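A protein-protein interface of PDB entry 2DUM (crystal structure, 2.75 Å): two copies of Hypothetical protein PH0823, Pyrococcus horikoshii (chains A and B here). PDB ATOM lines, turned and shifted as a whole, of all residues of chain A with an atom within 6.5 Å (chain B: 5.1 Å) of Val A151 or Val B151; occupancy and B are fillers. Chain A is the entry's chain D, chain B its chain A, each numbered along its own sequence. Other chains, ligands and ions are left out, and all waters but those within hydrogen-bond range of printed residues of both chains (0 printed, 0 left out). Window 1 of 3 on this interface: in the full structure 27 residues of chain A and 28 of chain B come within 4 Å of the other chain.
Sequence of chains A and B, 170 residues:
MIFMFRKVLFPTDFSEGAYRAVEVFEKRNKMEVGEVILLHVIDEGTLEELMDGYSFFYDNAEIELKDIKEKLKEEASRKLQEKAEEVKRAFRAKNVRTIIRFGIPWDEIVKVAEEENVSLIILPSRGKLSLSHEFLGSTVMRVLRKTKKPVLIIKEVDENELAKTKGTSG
Printed residues of chain A that touch a printed residue of chain B: Leu A120, Leu A144, Pro A150, Val A151, Leu A152, Ile A153 and Lys A155.
Hydrophobic or aromatic side chains of chain A that line the printed part of chain B: Leu A120, Leu A144, Pro A150 and Leu A152.
Among the printed residues, 14 pairs touch across the chains.
Among the printed residues, no Asp or Glu carboxylate lies within 4 Å of a Lys or Arg side-chain nitrogen of the other chain.
Leu A120 touches Leu B152.
Leu A144 touches Leu B144 (CD1 to CD1, 3.7 Å).
Leu A144 touches Ile B153 (CD2 to CD1, 3.8 Å).
Ile B153 touches Pro A150.
Leu B152 touches Val A151.
CD1 of Leu A152 touches CD1 of Leu B120, at 3.5 Å.
CD1 of Leu A152 touches CB of Pro B150, 3.96 Å away.
Leu A152 touches Val B151.
Ile A153 touches Pro B150.
Of chain B, only Val B151 (3.4 Å), Leu B152 (3.5 Å) and Ile B153 (2.7 Å) come within 4 Å of Val A151.
Of the printed residues of chain B, Leu A144 touches Leu B144 and Ile B153.
Of the printed residues of chain A, Thr B147 touches Lys A155 (2.5 Å).
Of the printed residues of chain B, Leu A152 touches Leu B120 (3.5 Å), Pro B150 (3.96 Å) and Val B151 (3.0 Å).
The nearest printed residue of chain B that does not touch Val A151 is Leu B123 (7.0 Å).
The nearest residue of chain A that does not touch Val B151 is Ile A154 (5.4 Å).
Leu B144 touches its own counterpart, Leu A144.
Val A151 touches its own counterpart, Val B151.
Val A151 touches Leu B152, and with the chains exchanged Leu A152 touches Val B151.
Leu A152 touches Pro B150, but with the chains exchanged Pro A150 does not touch Leu B152 (4.3 Å).
Positions printed for both chains: 120, 121, 123, 144, 147, 149, 150, 151, 152 and 153.
N of Leu A152 is in hydrogen-bond range of O of Ile A121 (3.0 Å).
N of Leu B152 is in hydrogen-bond range of O of Ile B121 (2.7 Å).
N of Ile A121 lies within hydrogen-bond range of O of Pro A150 (3.0 Å).
The backbone NH of Leu A123 is in hydrogen-bond range of the backbone carbonyl oxygen of Leu A152.
The backbone NH of Leu B123 is in hydrogen-bond range of the backbone carbonyl oxygen of Leu B152 (2.8 Å).
The backbone carbonyl oxygen (O) of Pro B150 sits at hydrogen-bond distance from the backbone NH (N) of Ile B121 (2.9 Å).
The backbone carbonyl oxygen (O) of Thr B147 lies within hydrogen-bond range of the side-chain amino group (NZ) of Lys A155 (2.5 Å).
The backbone NH of Ile A153 sits at hydrogen-bond distance from the backbone carbonyl oxygen of Val B151 (3.0 Å).
NZ of Lys A155 lies within hydrogen-bond range of O of Leu B144 (2.7 Å).
The backbone carbonyl oxygen (O) of Val A151 is in hydrogen-bond range of the backbone NH (N) of Ile B153 (2.7 Å).
The backbone carbonyl oxygen (O) of Val A151 sits close to the backbone carbonyl oxygen (O) of Val B151 (3.4 Å).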
ATOM      1  N   MET A   4     -23.024  26.626 -26.249  1.00  0.00           N
ATOM      2  CA  MET A   4     -23.146  25.095 -26.088  1.00  0.00           C
ATOM      3  C   MET A   4     -23.225  23.930 -27.184  1.00  0.00           C
ATOM      4  O   MET A   4     -23.229  22.722 -26.792  1.00  0.00           O
ATOM      5  CB  MET A   4     -24.200  24.684 -25.025  1.00  0.00           C
ATOM      6  CG  MET A   4     -24.021  23.133 -24.499  1.00  0.00           C
ATOM      7  SD  MET A   4     -24.469  22.820 -22.774  1.00  0.00           S
ATOM      8  CE  MET A   4     -23.220  21.767 -22.222  1.00  0.00           C
ATOM      9  N   LEU A 120     -19.802  19.346 -25.700  1.00  0.00           N
ATOM     10  CA  LEU A 120     -20.886  18.429 -25.396  1.00  0.00           C
ATOM     11  C   LEU A 120     -20.651  17.149 -26.170  1.00  0.00           C
ATOM     12  O   LEU A 120     -19.992  17.177 -27.234  1.00  0.00           O
ATOM     13  CB  LEU A 120     -22.178  19.016 -25.904  1.00  0.00           C
ATOM     14  CG  LEU A 120     -23.396  18.171 -26.198  1.00  0.00           C
ATOM     15  CD1 LEU A 120     -24.287  17.884 -24.872  1.00  0.00           C
ATOM     16  CD2 LEU A 120     -24.189  18.800 -27.292  1.00  0.00           C
ATOM     17  N   ILE A 121     -21.217  16.036 -25.685  1.00  0.00           N
ATOM     18  CA  ILE A 121     -21.098  14.756 -26.415  1.00  0.00           C
ATOM     19  C   ILE A 121     -22.451  14.214 -26.720  1.00  0.00           C
ATOM     20  O   ILE A 121     -23.278  14.160 -25.815  1.00  0.00           O
ATOM     21  CB  ILE A 121     -20.367  13.721 -25.577  1.00  0.00           C
ATOM     22  CG1 ILE A 121     -18.944  14.249 -25.310  1.00  0.00           C
ATOM     23  CG2 ILE A 121     -20.435  12.413 -26.266  1.00  0.00           C
ATOM     24  CD1 ILE A 121     -18.242  13.742 -23.962  1.00  0.00           C
ATOM     25  N   ILE A 122     -22.669  13.797 -27.963  1.00  0.00           N
ATOM     26  CA  ILE A 122     -24.002  13.363 -28.369  1.00  0.00           C
ATOM     27  C   ILE A 122     -23.974  11.904 -28.693  1.00  0.00           C
ATOM     28  O   ILE A 122     -23.432  11.486 -29.702  1.00  0.00           O
ATOM     29  CB  ILE A 122     -24.454  14.099 -29.586  1.00  0.00           C
ATOM     30  CG1 ILE A 122     -24.006  15.541 -29.460  1.00  0.00           C
ATOM     31  CG2 ILE A 122     -25.915  14.117 -29.646  1.00  0.00           C
ATOM     32  CD1 ILE A 122     -24.654  16.545 -30.451  1.00  0.00           C
ATOM     33  N   LEU A 123     -24.543  11.124 -27.804  1.00  0.00           N
ATOM     34  CA  LEU A 123     -24.607   9.668 -27.945  1.00  0.00           C
ATOM     35  C   LEU A 123     -25.981   9.178 -28.373  1.00  0.00           C
ATOM     36  O   LEU A 123     -27.019   9.607 -27.809  1.00  0.00           O
ATOM     37  CB  LEU A 123     -24.342   8.984 -26.612  1.00  0.00           C
ATOM     38  CG  LEU A 123     -22.965   8.468 -26.202  1.00  0.00           C
ATOM     39  CD1 LEU A 123     -21.947   8.394 -27.344  1.00  0.00           C
ATOM     40  CD2 LEU A 123     -22.523   9.376 -25.238  1.00  0.00           C
ATOM     41  N   VAL A 140     -22.508   3.825 -23.767  1.00  0.00           N
ATOM     42  CA  VAL A 140     -23.167   5.085 -23.373  1.00  0.00           C
ATOM     43  C   VAL A 140     -23.291   5.254 -21.868  1.00  0.00           C
ATOM     44  O   VAL A 140     -22.698   6.183 -21.315  1.00  0.00           O
ATOM     45  CB  VAL A 140     -24.514   5.352 -24.073  1.00  0.00           C
ATOM     46  CG1 VAL A 140     -25.048   4.095 -24.698  1.00  0.00           C
ATOM     47  CG2 VAL A 140     -25.497   6.016 -23.123  1.00  0.00           C
ATOM     48  N   VAL A 143     -19.558   6.042 -20.579  1.00  0.00           N
ATOM     49  CA  VAL A 143     -18.953   7.358 -20.934  1.00  0.00           C
ATOM     50  C   VAL A 143     -19.641   8.304 -20.029  1.00  0.00           C
ATOM     51  O   VAL A 143     -19.037   9.287 -19.517  1.00  0.00           O
ATOM     52  CB  VAL A 143     -19.303   7.849 -22.389  1.00  0.00           C
ATOM     53  CG1 VAL A 143     -18.343   7.375 -23.417  1.00  0.00           C
ATOM     54  CG2 VAL A 143     -20.504   7.284 -22.781  1.00  0.00           C
ATOM     55  N   LEU A 144     -20.920   7.956 -19.822  1.00  0.00           N
ATOM     56  CA  LEU A 144     -21.882   8.729 -19.092  1.00  0.00           C
ATOM     57  C   LEU A 144     -21.611   8.843 -17.610  1.00  0.00           C
ATOM     58  O   LEU A 144     -22.494   9.132 -16.843  1.00  0.00           O
ATOM     59  CB  LEU A 144     -23.240   8.098 -19.246  1.00  0.00           C
ATOM     60  CG  LEU A 144     -24.329   9.106 -19.519  1.00  0.00           C
ATOM     61  CD1 LEU A 144     -25.557   8.719 -18.770  1.00  0.00           C
ATOM     62  CD2 LEU A 144     -23.913  10.529 -19.155  1.00  0.00           C
ATOM     63  N   THR A 147     -17.135  10.605 -17.842  1.00  0.00           N
ATOM     64  CA  THR A 147     -16.749  11.915 -18.423  1.00  0.00           C
ATOM     65  C   THR A 147     -17.095  13.173 -17.675  1.00  0.00           C
ATOM     66  O   THR A 147     -18.154  13.345 -17.089  1.00  0.00           O
ATOM     67  CB  THR A 147     -17.254  12.179 -19.824  1.00  0.00           C
ATOM     68  OG1 THR A 147     -16.345  13.131 -20.416  1.00  0.00           O
ATOM     69  CG2 THR A 147     -18.614  12.765 -19.785  1.00  0.00           C
ATOM     70  N   LYS A 149     -17.393  16.174 -19.369  1.00  0.00           N
ATOM     71  CA  LYS A 149     -18.138  16.951 -20.364  1.00  0.00           C
ATOM     72  C   LYS A 149     -19.678  16.729 -20.174  1.00  0.00           C
ATOM     73  O   LYS A 149     -20.125  15.847 -19.383  1.00  0.00           O
ATOM     74  CB  LYS A 149     -17.614  16.596 -21.795  1.00  0.00           C
ATOM     75  CG  LYS A 149     -16.172  17.088 -22.169  1.00  0.00           C
ATOM     76  CD  LYS A 149     -15.673  18.120 -21.186  1.00  0.00           C
ATOM     77  CE  LYS A 149     -15.121  19.405 -21.809  1.00  0.00           C
ATOM     78  NZ  LYS A 149     -13.809  19.136 -22.599  1.00  0.00           N
ATOM     79  N   PRO A 150     -20.519  17.594 -20.742  1.00  0.00           N
ATOM     80  CA  PRO A 150     -21.902  17.206 -20.595  1.00  0.00           C
ATOM     81  C   PRO A 150     -22.307  16.355 -21.749  1.00  0.00           C
ATOM     82  O   PRO A 150     -21.580  16.309 -22.709  1.00  0.00           O
ATOM     83  CB  PRO A 150     -22.617  18.529 -20.609  1.00  0.00           C
ATOM     84  CG  PRO A 150     -21.466  19.603 -20.571  1.00  0.00           C
ATOM     85  CD  PRO A 150     -20.402  18.952 -21.272  1.00  0.00           C
ATOM     86  N   VAL A 151     -23.420  15.643 -21.632  1.00  0.00           N
ATOM     87  CA  VAL A 151     -23.790  14.730 -22.633  1.00  0.00           C
ATOM     88  C   VAL A 151     -25.277  14.651 -22.798  1.00  0.00           C
ATOM     89  O   VAL A 151     -26.053  14.826 -21.890  1.00  0.00           O
ATOM     90  CB  VAL A 151     -23.139  13.336 -22.468  1.00  0.00           C
ATOM     91  CG1 VAL A 151     -22.032  13.338 -21.474  1.00  0.00           C
ATOM     92  CG2 VAL A 151     -24.150  12.305 -22.062  1.00  0.00           C
ATOM     93  N   LEU A 152     -25.647  14.462 -24.045  1.00  0.00           N
ATOM     94  CA  LEU A 152     -26.983  14.639 -24.553  1.00  0.00           C
ATOM     95  C   LEU A 152     -27.182  13.390 -25.269  1.00  0.00           C
ATOM     96  O   LEU A 152     -26.470  13.117 -26.277  1.00  0.00           O
ATOM     97  CB  LEU A 152     -27.052  15.713 -25.626  1.00  0.00           C
ATOM     98  CG  LEU A 152     -28.380  15.493 -26.389  1.00  0.00           C
ATOM     99  CD1 LEU A 152     -29.500  15.980 -25.605  1.00  0.00           C
ATOM    100  CD2 LEU A 152     -28.493  16.164 -27.710  1.00  0.00           C
ATOM    101  N   ILE A 153     -28.147  12.637 -24.782  1.00  0.00           N
ATOM    102  CA  ILE A 153     -28.424  11.319 -25.317  1.00  0.00           C
ATOM    103  C   ILE A 153     -29.578  11.438 -26.251  1.00  0.00           C
ATOM    104  O   ILE A 153     -30.567  12.051 -25.941  1.00  0.00           O
ATOM    105  CB  ILE A 153     -28.798  10.324 -24.194  1.00  0.00           C
ATOM    106  CG1 ILE A 153     -27.565   9.780 -23.564  1.00  0.00           C
ATOM    107  CG2 ILE A 153     -29.402   9.181 -24.741  1.00  0.00           C
ATOM    108  CD1 ILE A 153     -27.283  10.615 -22.412  1.00  0.00           C
ATOM    109  N   ILE A 154     -29.530  10.832 -27.401  1.00  0.00           N
ATOM    110  CA  ILE A 154     -30.786  10.932 -28.078  1.00  0.00           C
ATOM    111  C   ILE A 154     -31.372   9.628 -28.560  1.00  0.00           C
ATOM    112  O   ILE A 154     -30.668   8.684 -28.976  1.00  0.00           O
ATOM    113  CB  ILE A 154     -30.873  12.123 -29.095  1.00  0.00           C
ATOM    114  CG1 ILE A 154     -30.486  11.687 -30.477  1.00  0.00           C
ATOM    115  CG2 ILE A 154     -29.925  13.239 -28.685  1.00  0.00           C
ATOM    116  CD1 ILE A 154     -29.308  12.598 -31.035  1.00  0.00           C
ATOM    117  N   LYS A 155     -32.697   9.614 -28.473  1.00  0.00           N
ATOM    118  CA  LYS A 155     -33.482   8.482 -28.861  1.00  0.00           C
ATOM    119  C   LYS A 155     -33.997   8.514 -30.325  1.00  0.00           C
ATOM    120  O   LYS A 155     -33.183   8.344 -31.270  1.00  0.00           O
ATOM    121  CB  LYS A 155     -34.570   8.263 -27.797  1.00  0.00           C
ATOM    122  CG  LYS A 155     -34.005   8.096 -26.358  1.00  0.00           C
ATOM    123  CD  LYS A 155     -34.995   7.378 -25.463  1.00  0.00           C
ATOM    124  CE  LYS A 155     -34.304   6.794 -24.257  1.00  0.00           C
ATOM    125  NZ  LYS A 155     -35.023   7.063 -23.001  1.00  0.00           N
ATOM    126  N   LEU B 120     -36.247  19.157 -25.143  1.00  0.00           N
ATOM    127  CA  LEU B 120     -35.155  18.587 -24.442  1.00  0.00           C
ATOM    128  C   LEU B 120     -35.555  18.448 -23.013  1.00  0.00           C
ATOM    129  O   LEU B 120     -36.373  19.231 -22.519  1.00  0.00           O
ATOM    130  CB  LEU B 120     -33.993  19.548 -24.431  1.00  0.00           C
ATOM    131  CG  LEU B 120     -32.701  19.010 -23.828  1.00  0.00           C
ATOM    132  CD1 LEU B 120     -32.337  17.616 -24.300  1.00  0.00           C
ATOM    133  CD2 LEU B 120     -31.539  19.827 -24.234  1.00  0.00           C
ATOM    134  N   ILE B 121     -34.968  17.468 -22.312  1.00  0.00           N
ATOM    135  CA  ILE B 121     -34.915  17.597 -20.848  1.00  0.00           C
ATOM    136  C   ILE B 121     -33.491  17.773 -20.366  1.00  0.00           C
ATOM    137  O   ILE B 121     -32.592  17.141 -20.925  1.00  0.00           O
ATOM    138  CB  ILE B 121     -35.832  16.642 -19.971  1.00  0.00           C
ATOM    139  CG1 ILE B 121     -34.987  16.027 -18.918  1.00  0.00           C
ATOM    140  CG2 ILE B 121     -36.481  15.510 -20.682  1.00  0.00           C
ATOM    141  CD1 ILE B 121     -35.551  16.104 -17.551  1.00  0.00           C
ATOM    142  N   LEU B 123     -31.012  17.841 -16.988  1.00  0.00           N
ATOM    143  CA  LEU B 123     -30.858  17.317 -15.623  1.00  0.00           C
ATOM    144  C   LEU B 123     -29.445  17.481 -15.072  1.00  0.00           C
ATOM    145  O   LEU B 123     -28.451  17.305 -15.829  1.00  0.00           O
ATOM    146  CB  LEU B 123     -30.947  15.818 -15.631  1.00  0.00           C
ATOM    147  CG  LEU B 123     -32.185  15.016 -15.606  1.00  0.00           C
ATOM    148  CD1 LEU B 123     -33.141  16.054 -15.205  1.00  0.00           C
ATOM    149  CD2 LEU B 123     -32.448  14.494 -16.987  1.00  0.00           C
ATOM    150  N   LEU B 144     -33.723   9.092 -17.729  1.00  0.00           N
ATOM    151  CA  LEU B 144     -32.908   8.584 -18.812  1.00  0.00           C
ATOM    152  C   LEU B 144     -33.523   7.443 -19.591  1.00  0.00           C
ATOM    153  O   LEU B 144     -33.561   7.481 -20.818  1.00  0.00           O
ATOM    154  CB  LEU B 144     -31.586   8.114 -18.309  1.00  0.00           C
ATOM    155  CG  LEU B 144     -30.675   8.974 -19.121  1.00  0.00           C
ATOM    156  CD1 LEU B 144     -29.245   8.871 -18.626  1.00  0.00           C
ATOM    157  CD2 LEU B 144     -30.797   8.581 -20.533  1.00  0.00           C
ATOM    158  N   THR B 147     -37.847   7.894 -20.757  1.00  0.00           N
ATOM    159  CA  THR B 147     -38.276   8.942 -21.679  1.00  0.00           C
ATOM    160  C   THR B 147     -38.045   8.681 -23.178  1.00  0.00           C
ATOM    161  O   THR B 147     -37.315   7.770 -23.529  1.00  0.00           O
ATOM    162  CB  THR B 147     -37.723  10.259 -21.254  1.00  0.00           C
ATOM    163  OG1 THR B 147     -38.544  11.251 -21.810  1.00  0.00           O
ATOM    164  CG2 THR B 147     -36.306  10.486 -21.704  1.00  0.00           C
ATOM    165  N   LYS B 149     -38.132  11.758 -25.329  1.00  0.00           N
ATOM    166  CA  LYS B 149     -37.413  13.021 -25.360  1.00  0.00           C
ATOM    167  C   LYS B 149     -35.809  12.885 -25.295  1.00  0.00           C
ATOM    168  O   LYS B 149     -35.266  11.818 -24.869  1.00  0.00           O
ATOM    169  CB  LYS B 149     -38.035  13.924 -24.268  1.00  0.00           C
ATOM    170  CG  LYS B 149     -39.241  14.817 -24.678  1.00  0.00           C
ATOM    171  CD  LYS B 149     -40.438  14.061 -25.146  1.00  0.00           C
ATOM    172  CE  LYS B 149     -41.494  14.989 -25.658  1.00  0.00           C
ATOM    173  NZ  LYS B 149     -41.002  15.862 -26.825  1.00  0.00           N
ATOM    174  N   PRO B 150     -35.058  13.890 -25.850  1.00  0.00           N
ATOM    175  CA  PRO B 150     -33.598  13.955 -25.631  1.00  0.00           C
ATOM    176  C   PRO B 150     -33.237  14.486 -24.278  1.00  0.00           C
ATOM    177  O   PRO B 150     -34.139  14.998 -23.585  1.00  0.00           O
ATOM    178  CB  PRO B 150     -33.101  14.816 -26.770  1.00  0.00           C
ATOM    179  CG  PRO B 150     -34.260  15.652 -27.192  1.00  0.00           C
ATOM    180  CD  PRO B 150     -35.517  14.880 -26.845  1.00  0.00           C
ATOM    181  N   VAL B 151     -31.987  14.270 -23.835  1.00  0.00           N
ATOM    182  CA  VAL B 151     -31.667  14.524 -22.430  1.00  0.00           C
ATOM    183  C   VAL B 151     -30.292  15.074 -22.223  1.00  0.00           C
ATOM    184  O   VAL B 151     -29.329  14.460 -22.646  1.00  0.00           O
ATOM    185  CB  VAL B 151     -31.789  13.276 -21.534  1.00  0.00           C
ATOM    186  CG1 VAL B 151     -31.295  13.577 -20.064  1.00  0.00           C
ATOM    187  CG2 VAL B 151     -33.199  12.787 -21.439  1.00  0.00           C
ATOM    188  N   LEU B 152     -30.175  16.209 -21.541  1.00  0.00           N
ATOM    189  CA  LEU B 152     -28.880  16.787 -21.348  1.00  0.00           C
ATOM    190  C   LEU B 152     -28.462  16.481 -19.901  1.00  0.00           C
ATOM    191  O   LEU B 152     -29.082  16.923 -18.852  1.00  0.00           O
ATOM    192  CB  LEU B 152     -28.993  18.286 -21.571  1.00  0.00           C
ATOM    193  CG  LEU B 152     -27.899  18.986 -22.389  1.00  0.00           C
ATOM    194  CD1 LEU B 152     -27.839  20.422 -22.087  1.00  0.00           C
ATOM    195  CD2 LEU B 152     -26.622  18.522 -22.082  1.00  0.00           C
ATOM    196  N   ILE B 153     -27.411  15.704 -19.765  1.00  0.00           N
ATOM    197  CA  ILE B 153     -27.003  15.604 -18.379  1.00  0.00           C
ATOM    198  C   ILE B 153     -25.804  16.503 -18.150  1.00  0.00           C
ATOM    199  O   ILE B 153     -24.748  16.356 -18.769  1.00  0.00           O
ATOM    200  CB  ILE B 153     -27.004  14.174 -17.733  1.00  0.00           C
ATOM    201  CG1 ILE B 153     -25.900  14.159 -16.725  1.00  0.00           C
ATOM    202  CG2 ILE B 153     -26.886  13.031 -18.689  1.00  0.00           C
ATOM    203  CD1 ILE B 153     -24.415  13.886 -17.390  1.00  0.00           C
